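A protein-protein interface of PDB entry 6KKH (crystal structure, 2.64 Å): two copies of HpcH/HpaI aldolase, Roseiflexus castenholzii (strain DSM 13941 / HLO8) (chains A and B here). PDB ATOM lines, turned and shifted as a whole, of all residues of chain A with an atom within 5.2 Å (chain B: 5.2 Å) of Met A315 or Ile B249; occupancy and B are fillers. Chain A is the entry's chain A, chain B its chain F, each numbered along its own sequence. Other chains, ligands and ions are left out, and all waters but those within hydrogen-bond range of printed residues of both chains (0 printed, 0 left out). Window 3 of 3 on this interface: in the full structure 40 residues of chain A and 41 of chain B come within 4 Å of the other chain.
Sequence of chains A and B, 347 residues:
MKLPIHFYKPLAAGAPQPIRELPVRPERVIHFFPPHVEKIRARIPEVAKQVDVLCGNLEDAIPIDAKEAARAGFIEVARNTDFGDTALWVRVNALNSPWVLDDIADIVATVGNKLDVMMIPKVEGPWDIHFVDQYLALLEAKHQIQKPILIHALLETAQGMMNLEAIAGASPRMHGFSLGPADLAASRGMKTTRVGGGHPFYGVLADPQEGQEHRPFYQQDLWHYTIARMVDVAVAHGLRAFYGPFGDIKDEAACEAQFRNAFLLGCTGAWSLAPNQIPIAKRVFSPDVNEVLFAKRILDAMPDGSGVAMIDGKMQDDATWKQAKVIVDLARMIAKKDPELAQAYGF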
ATOM      1  N   VAL A 308      -7.637 -19.488 -37.974  1.00  0.00           N
ATOM      2  CA  VAL A 308      -7.580 -18.886 -36.608  1.00  0.00           C
ATOM      3  C   VAL A 308      -8.165 -17.469 -36.674  1.00  0.00           C
ATOM      4  O   VAL A 308      -8.217 -16.892 -37.772  1.00  0.00           O
ATOM      5  CB  VAL A 308      -6.137 -18.844 -36.079  1.00  0.00           C
ATOM      6  CG1 VAL A 308      -6.094 -18.461 -34.619  1.00  0.00           C
ATOM      7  CG2 VAL A 308      -5.422 -20.160 -36.283  1.00  0.00           C
ATOM      8  N   ALA A 309      -8.640 -16.928 -35.552  1.00  0.00           N
ATOM      9  CA  ALA A 309      -9.186 -15.569 -35.574  1.00  0.00           C
ATOM     10  C   ALA A 309      -8.994 -14.934 -34.191  1.00  0.00           C
ATOM     11  O   ALA A 309      -9.264 -15.578 -33.173  1.00  0.00           O
ATOM     12  CB  ALA A 309     -10.640 -15.594 -35.983  1.00  0.00           C
ATOM     13  N   MET A 310      -8.522 -13.681 -34.174  1.00  0.00           N
ATOM     14  CA  MET A 310      -8.208 -12.927 -32.940  1.00  0.00           C
ATOM     15  C   MET A 310      -7.097 -13.655 -32.164  1.00  0.00           C
ATOM     16  O   MET A 310      -7.114 -13.762 -30.930  1.00  0.00           O
ATOM     17  CB  MET A 310      -9.446 -12.749 -32.050  1.00  0.00           C
ATOM     18  CG  MET A 310     -10.687 -12.247 -32.784  1.00  0.00           C
ATOM     19  SD  MET A 310     -12.153 -12.142 -31.706  1.00  0.00           S
ATOM     20  CE  MET A 310     -13.474 -12.293 -32.908  1.00  0.00           C
ATOM     21  N   GLY A 313     -10.919 -10.455 -28.577  1.00  0.00           N
ATOM     22  CA  GLY A 313      -9.680 -10.884 -27.936  1.00  0.00           C
ATOM     23  C   GLY A 313      -9.757 -12.322 -27.443  1.00  0.00           C
ATOM     24  O   GLY A 313      -9.137 -12.674 -26.427  1.00  0.00           O
ATOM     25  N   LYS A 314     -10.516 -13.149 -28.171  1.00  0.00           N
ATOM     26  CA  LYS A 314     -10.725 -14.563 -27.833  1.00  0.00           C
ATOM     27  C   LYS A 314     -10.356 -15.430 -29.044  1.00  0.00           C
ATOM     28  O   LYS A 314     -10.723 -15.110 -30.174  1.00  0.00           O
ATOM     29  CB  LYS A 314     -12.179 -14.801 -27.413  1.00  0.00           C
ATOM     30  CG  LYS A 314     -12.510 -14.422 -25.976  1.00  0.00           C
ATOM     31  CD  LYS A 314     -13.987 -14.176 -25.733  1.00  0.00           C
ATOM     32  CE  LYS A 314     -14.278 -13.652 -24.343  1.00  0.00           C
ATOM     33  NZ  LYS A 314     -15.660 -13.130 -24.233  1.00  0.00           N
ATOM     34  N   MET A 315      -9.641 -16.526 -28.795  1.00  0.00           N
ATOM     35  CA  MET A 315      -9.146 -17.389 -29.869  1.00  0.00           C
ATOM     36  C   MET A 315     -10.296 -18.241 -30.423  1.00  0.00           C
ATOM     37  O   MET A 315     -10.953 -18.978 -29.684  1.00  0.00           O
ATOM     38  CB  MET A 315      -8.028 -18.314 -29.372  1.00  0.00           C
ATOM     39  CG  MET A 315      -7.272 -19.007 -30.497  1.00  0.00           C
ATOM     40  SD  MET A 315      -6.684 -20.663 -30.050  1.00  0.00           S
ATOM     41  CE  MET A 315      -8.234 -21.558 -29.944  1.00  0.00           C
ATOM     42  N   GLN A 316     -10.513 -18.122 -31.730  1.00  0.00           N
ATOM     43  CA  GLN A 316     -11.466 -18.951 -32.472  1.00  0.00           C
ATOM     44  C   GLN A 316     -10.680 -19.948 -33.335  1.00  0.00           C
ATOM     45  O   GLN A 316      -9.457 -19.836 -33.457  1.00  0.00           O
ATOM     46  CB  GLN A 316     -12.376 -18.067 -33.331  1.00  0.00           C
ATOM     47  CG  GLN A 316     -13.712 -17.723 -32.682  1.00  0.00           C
ATOM     48  CD  GLN A 316     -13.580 -17.120 -31.306  1.00  0.00           C
ATOM     49  OE1 GLN A 316     -14.199 -17.573 -30.343  1.00  0.00           O
ATOM     50  NE2 GLN A 316     -12.767 -16.081 -31.203  1.00  0.00           N
ATOM     51  N   ASP A 317     -11.384 -20.921 -33.915  1.00  0.00           N
ATOM     52  CA  ASP A 317     -10.774 -21.903 -34.826  1.00  0.00           C
ATOM     53  C   ASP A 317     -11.890 -22.720 -35.500  1.00  0.00           C
ATOM     54  O   ASP A 317     -13.032 -22.258 -35.586  1.00  0.00           O
ATOM     55  CB  ASP A 317      -9.729 -22.762 -34.097  1.00  0.00           C
ATOM     56  CG  ASP A 317     -10.202 -23.394 -32.797  1.00  0.00           C
ATOM     57  OD1 ASP A 317      -9.346 -23.937 -32.070  1.00  0.00           O
ATOM     58  OD2 ASP A 317     -11.415 -23.335 -32.519  1.00  0.00           O
ATOM     59  N   THR A 320     -14.674 -23.599 -32.695  1.00  0.00           N
ATOM     60  CA  THR A 320     -15.603 -22.489 -32.433  1.00  0.00           C
ATOM     61  C   THR A 320     -16.513 -22.252 -33.643  1.00  0.00           C
ATOM     62  O   THR A 320     -17.642 -21.801 -33.477  1.00  0.00           O
ATOM     63  CB  THR A 320     -14.864 -21.189 -32.097  1.00  0.00           C
ATOM     64  OG1 THR A 320     -13.997 -20.908 -33.196  1.00  0.00           O
ATOM     65  CG2 THR A 320     -14.086 -21.260 -30.800  1.00  0.00           C
ATOM     66  N   VAL B 195     -14.861 -20.864 -25.122  1.00  0.00           N
ATOM     67  CA  VAL B 195     -13.933 -21.991 -25.086  1.00  0.00           C
ATOM     68  C   VAL B 195     -13.502 -22.239 -23.633  1.00  0.00           C
ATOM     69  O   VAL B 195     -12.330 -22.140 -23.276  1.00  0.00           O
ATOM     70  CB  VAL B 195     -12.735 -21.755 -26.028  1.00  0.00           C
ATOM     71  CG1 VAL B 195     -11.687 -22.855 -25.928  1.00  0.00           C
ATOM     72  CG2 VAL B 195     -13.195 -21.596 -27.469  1.00  0.00           C
ATOM     73  N   PHE B 246      -7.953 -22.545 -22.736  1.00  0.00           N
ATOM     74  CA  PHE B 246      -8.785 -21.445 -22.277  1.00  0.00           C
ATOM     75  C   PHE B 246      -8.690 -20.313 -23.302  1.00  0.00           C
ATOM     76  O   PHE B 246      -7.688 -19.606 -23.349  1.00  0.00           O
ATOM     77  CB  PHE B 246      -8.355 -20.993 -20.881  1.00  0.00           C
ATOM     78  CG  PHE B 246      -9.299 -20.001 -20.255  1.00  0.00           C
ATOM     79  CD1 PHE B 246     -10.472 -20.429 -19.653  1.00  0.00           C
ATOM     80  CD2 PHE B 246      -9.031 -18.642 -20.291  1.00  0.00           C
ATOM     81  CE1 PHE B 246     -11.351 -19.520 -19.086  1.00  0.00           C
ATOM     82  CE2 PHE B 246      -9.908 -17.732 -19.718  1.00  0.00           C
ATOM     83  CZ  PHE B 246     -11.066 -18.174 -19.118  1.00  0.00           C
ATOM     84  N   GLY B 247      -9.741 -20.154 -24.105  1.00  0.00           N
ATOM     85  CA  GLY B 247      -9.705 -19.332 -25.321  1.00  0.00           C
ATOM     86  C   GLY B 247      -9.689 -17.832 -25.052  1.00  0.00           C
ATOM     87  O   GLY B 247      -9.255 -17.066 -25.913  1.00  0.00           O
ATOM     88  N   ASP B 248     -10.170 -17.394 -23.886  1.00  0.00           N
ATOM     89  CA  ASP B 248     -10.093 -15.976 -23.514  1.00  0.00           C
ATOM     90  C   ASP B 248      -8.666 -15.675 -23.037  1.00  0.00           C
ATOM     91  O   ASP B 248      -8.363 -15.720 -21.841  1.00  0.00           O
ATOM     92  CB  ASP B 248     -11.156 -15.604 -22.473  1.00  0.00           C
ATOM     93  CG  ASP B 248     -11.489 -14.121 -22.434  1.00  0.00           C
ATOM     94  OD1 ASP B 248     -10.821 -13.349 -23.153  1.00  0.00           O
ATOM     95  OD2 ASP B 248     -12.414 -13.747 -21.682  1.00  0.00           O
ATOM     96  N   ILE B 249      -7.802 -15.364 -23.997  1.00  0.00           N
ATOM     97  CA  ILE B 249      -6.373 -15.192 -23.736  1.00  0.00           C
ATOM     98  C   ILE B 249      -6.171 -14.004 -22.783  1.00  0.00           C
ATOM     99  O   ILE B 249      -5.373 -14.085 -21.847  1.00  0.00           O
ATOM    100  CB  ILE B 249      -5.589 -15.015 -25.055  1.00  0.00           C
ATOM    101  CG1 ILE B 249      -5.688 -16.254 -25.950  1.00  0.00           C
ATOM    102  CG2 ILE B 249      -4.139 -14.645 -24.778  1.00  0.00           C
ATOM    103  CD1 ILE B 249      -5.494 -15.963 -27.422  1.00  0.00           C
ATOM    104  N   LYS B 250      -6.913 -12.924 -23.017  1.00  0.00           N
ATOM    105  CA  LYS B 250      -6.715 -11.667 -22.291  1.00  0.00           C
ATOM    106  C   LYS B 250      -7.110 -11.836 -20.814  1.00  0.00           C
ATOM    107  O   LYS B 250      -6.450 -11.286 -19.933  1.00  0.00           O
ATOM    108  CB  LYS B 250      -7.515 -10.537 -22.953  1.00  0.00           C
ATOM    109  CG  LYS B 250      -6.718  -9.274 -23.255  1.00  0.00           C
ATOM    110  CD  LYS B 250      -7.570  -8.085 -23.673  1.00  0.00           C
ATOM    111  CE  LYS B 250      -8.299  -7.435 -22.513  1.00  0.00           C
ATOM    112  NZ  LYS B 250      -8.801  -6.083 -22.857  1.00  0.00           N
ATOM    113  N   ASP B 251      -8.167 -12.603 -20.544  1.00  0.00           N
ATOM    114  CA  ASP B 251      -8.783 -12.653 -19.209  1.00  0.00           C
ATOM    115  C   ASP B 251      -8.007 -13.624 -18.307  1.00  0.00           C
ATOM    116  O   ASP B 251      -8.455 -14.735 -18.033  1.00  0.00           O
ATOM    117  CB  ASP B 251     -10.268 -13.016 -19.316  1.00  0.00           C
ATOM    118  CG  ASP B 251     -11.105 -12.569 -18.131  1.00  0.00           C
ATOM    119  OD1 ASP B 251     -10.566 -12.543 -17.006  1.00  0.00           O
ATOM    120  OD2 ASP B 251     -12.291 -12.253 -18.342  1.00  0.00           O
ATOM    121  N   GLU B 252      -6.863 -13.170 -17.812  1.00  0.00           N
ATOM    122  CA  GLU B 252      -5.975 -14.005 -17.010  1.00  0.00           C
ATOM    123  C   GLU B 252      -6.605 -14.298 -15.644  1.00  0.00           C
ATOM    124  O   GLU B 252      -6.221 -15.265 -14.985  1.00  0.00           O
ATOM    125  CB  GLU B 252      -4.627 -13.316 -16.790  1.00  0.00           C
ATOM    126  CG  GLU B 252      -3.906 -12.952 -18.076  1.00  0.00           C
ATOM    127  CD  GLU B 252      -2.444 -12.581 -17.892  1.00  0.00           C
ATOM    128  OE1 GLU B 252      -1.919 -12.787 -16.778  1.00  0.00           O
ATOM    129  OE2 GLU B 252      -1.835 -12.096 -18.865  1.00  0.00           O
ATOM    130  N   LEU B 273      -2.039 -21.243 -24.893  1.00  0.00           N
ATOM    131  CA  LEU B 273      -2.200 -20.875 -26.312  1.00  0.00           C
ATOM    132  C   LEU B 273      -1.418 -19.594 -26.637  1.00  0.00           C
ATOM    133  O   LEU B 273      -1.389 -19.164 -27.797  1.00  0.00           O
ATOM    134  CB  LEU B 273      -3.690 -20.682 -26.610  1.00  0.00           C
ATOM    135  CG  LEU B 273      -4.583 -21.899 -26.370  1.00  0.00           C
ATOM    136  CD1 LEU B 273      -6.037 -21.555 -26.653  1.00  0.00           C
ATOM    137  CD2 LEU B 273      -4.140 -23.085 -27.216  1.00  0.00           C
ATOM    138  N   ALA B 274      -0.801 -18.989 -25.620  1.00  0.00           N
ATOM    139  CA  ALA B 274       0.004 -17.773 -25.777  1.00  0.00           C
ATOM    140  C   ALA B 274       0.939 -17.638 -24.565  1.00  0.00           C
ATOM    141  O   ALA B 274       0.717 -18.294 -23.545  1.00  0.00           O
ATOM    142  CB  ALA B 274      -0.910 -16.580 -25.933  1.00  0.00           C
ATOM    143  N   ASN B 276       1.399 -15.642 -22.157  1.00  0.00           N
ATOM    144  CA  ASN B 276       0.872 -15.149 -20.881  1.00  0.00           C
ATOM    145  C   ASN B 276       0.270 -16.299 -20.062  1.00  0.00           C
ATOM    146  O   ASN B 276       0.148 -16.173 -18.840  1.00  0.00           O
ATOM    147  CB  ASN B 276      -0.142 -14.015 -21.081  1.00  0.00           C
ATOM    148  CG  ASN B 276      -1.293 -14.368 -22.001  1.00  0.00           C
ATOM    149  OD1 ASN B 276      -1.128 -15.135 -22.945  1.00  0.00           O
ATOM    150  ND2 ASN B 276      -2.459 -13.797 -21.749  1.00  0.00           N
ATOM    151  N   GLN B 277      -0.095 -17.408 -20.708  1.00  0.00           N
ATOM    152  CA  GLN B 277      -0.732 -18.536 -20.007  1.00  0.00           C
ATOM    153  C   GLN B 277       0.326 -19.503 -19.450  1.00  0.00           C
ATOM    154  O   GLN B 277       0.017 -20.263 -18.535  1.00  0.00           O
ATOM    155  CB  GLN B 277      -1.718 -19.252 -20.935  1.00  0.00           C
ATOM    156  CG  GLN B 277      -2.982 -18.448 -21.207  1.00  0.00           C
ATOM    157  CD  GLN B 277      -3.928 -19.119 -22.173  1.00  0.00           C
ATOM    158  OE1 GLN B 277      -3.524 -19.903 -23.027  1.00  0.00           O
ATOM    159  NE2 GLN B 277      -5.207 -18.801 -22.054  1.00  0.00           N
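Of the 12 printed residues of chain B, 5 touch a printed residue of chain A. Printed residues of chain B that touch a printed residue of chain A: Val B195, Gly B247, Asp B248, Ile B249 and Leu B273. Of the 9 printed residues of chain A, 4 touch a printed residue of chain B. Among the printed residues, no Asp or Glu carboxylate lies within 4 Å of a Lys or Arg side-chain nitrogen of the other chain.
N of Met A315 lies within hydrogen-bond range of O of Gly B247 (3.0 Å).
Met A315 touches just these residues of chain B: Gly B247 (3.0 Å), Ile B249 (3.97 Å) and Leu B273 (3.6 Å). Of chain A, only Gly A313 and Met A315 come within 4 Å of Ile B249. Of the printed residues of chain A, Asp B248 touches Gly A313 (3.7 Å) and Lys A314 (3.3 Å). Of the printed residues of chain A, Gly B247 touches Lys A314 and Met A315. The nearest residue of chain B that does not touch Met A315 is Val B195 (4.1 Å). The nearest printed residue of chain A that does not touch Asp B248 is Met A315 (5.0 Å).
Among the printed residues, merely in contact across the chains: Gly A313 with Asp B248 (3.7 Å), Gly A313 with Ile B249 (3.9 Å), Lys A314 with Gly B247 (3.5 Å), Lys A314 with Asp B248 (3.3 Å), Met A315 with Ile B249 (3.97 Å), Met A315 with Leu B273 (3.6 Å) and Thr A320 with Val B195 (3.5 Å).
No position is printed for both chains.
ND2 of Asn B276 lies within hydrogen-bond range of O of Ile B249. The backbone NH (N) of Leu B273 is in hydrogen-bond range of the side-chain amide oxygen (OE1) of Gln B277. N of Asp A317 lies within hydrogen-bond range of OG1 of Thr A320. The backbone NH of Gly B247 sits at hydrogen-bond distance from the backbone carbonyl oxygen of Val B195, at 3.4 Å. The backbone carbonyl oxygen of Lys A314 is in hydrogen-bond range of the side-chain amide nitrogen of Gln A316 (2.5 Å). The backbone NH (N) of Gly A313 lies within hydrogen-bond range of the side-chain sulfur (SD) of Met A310, at 3.8 Å.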
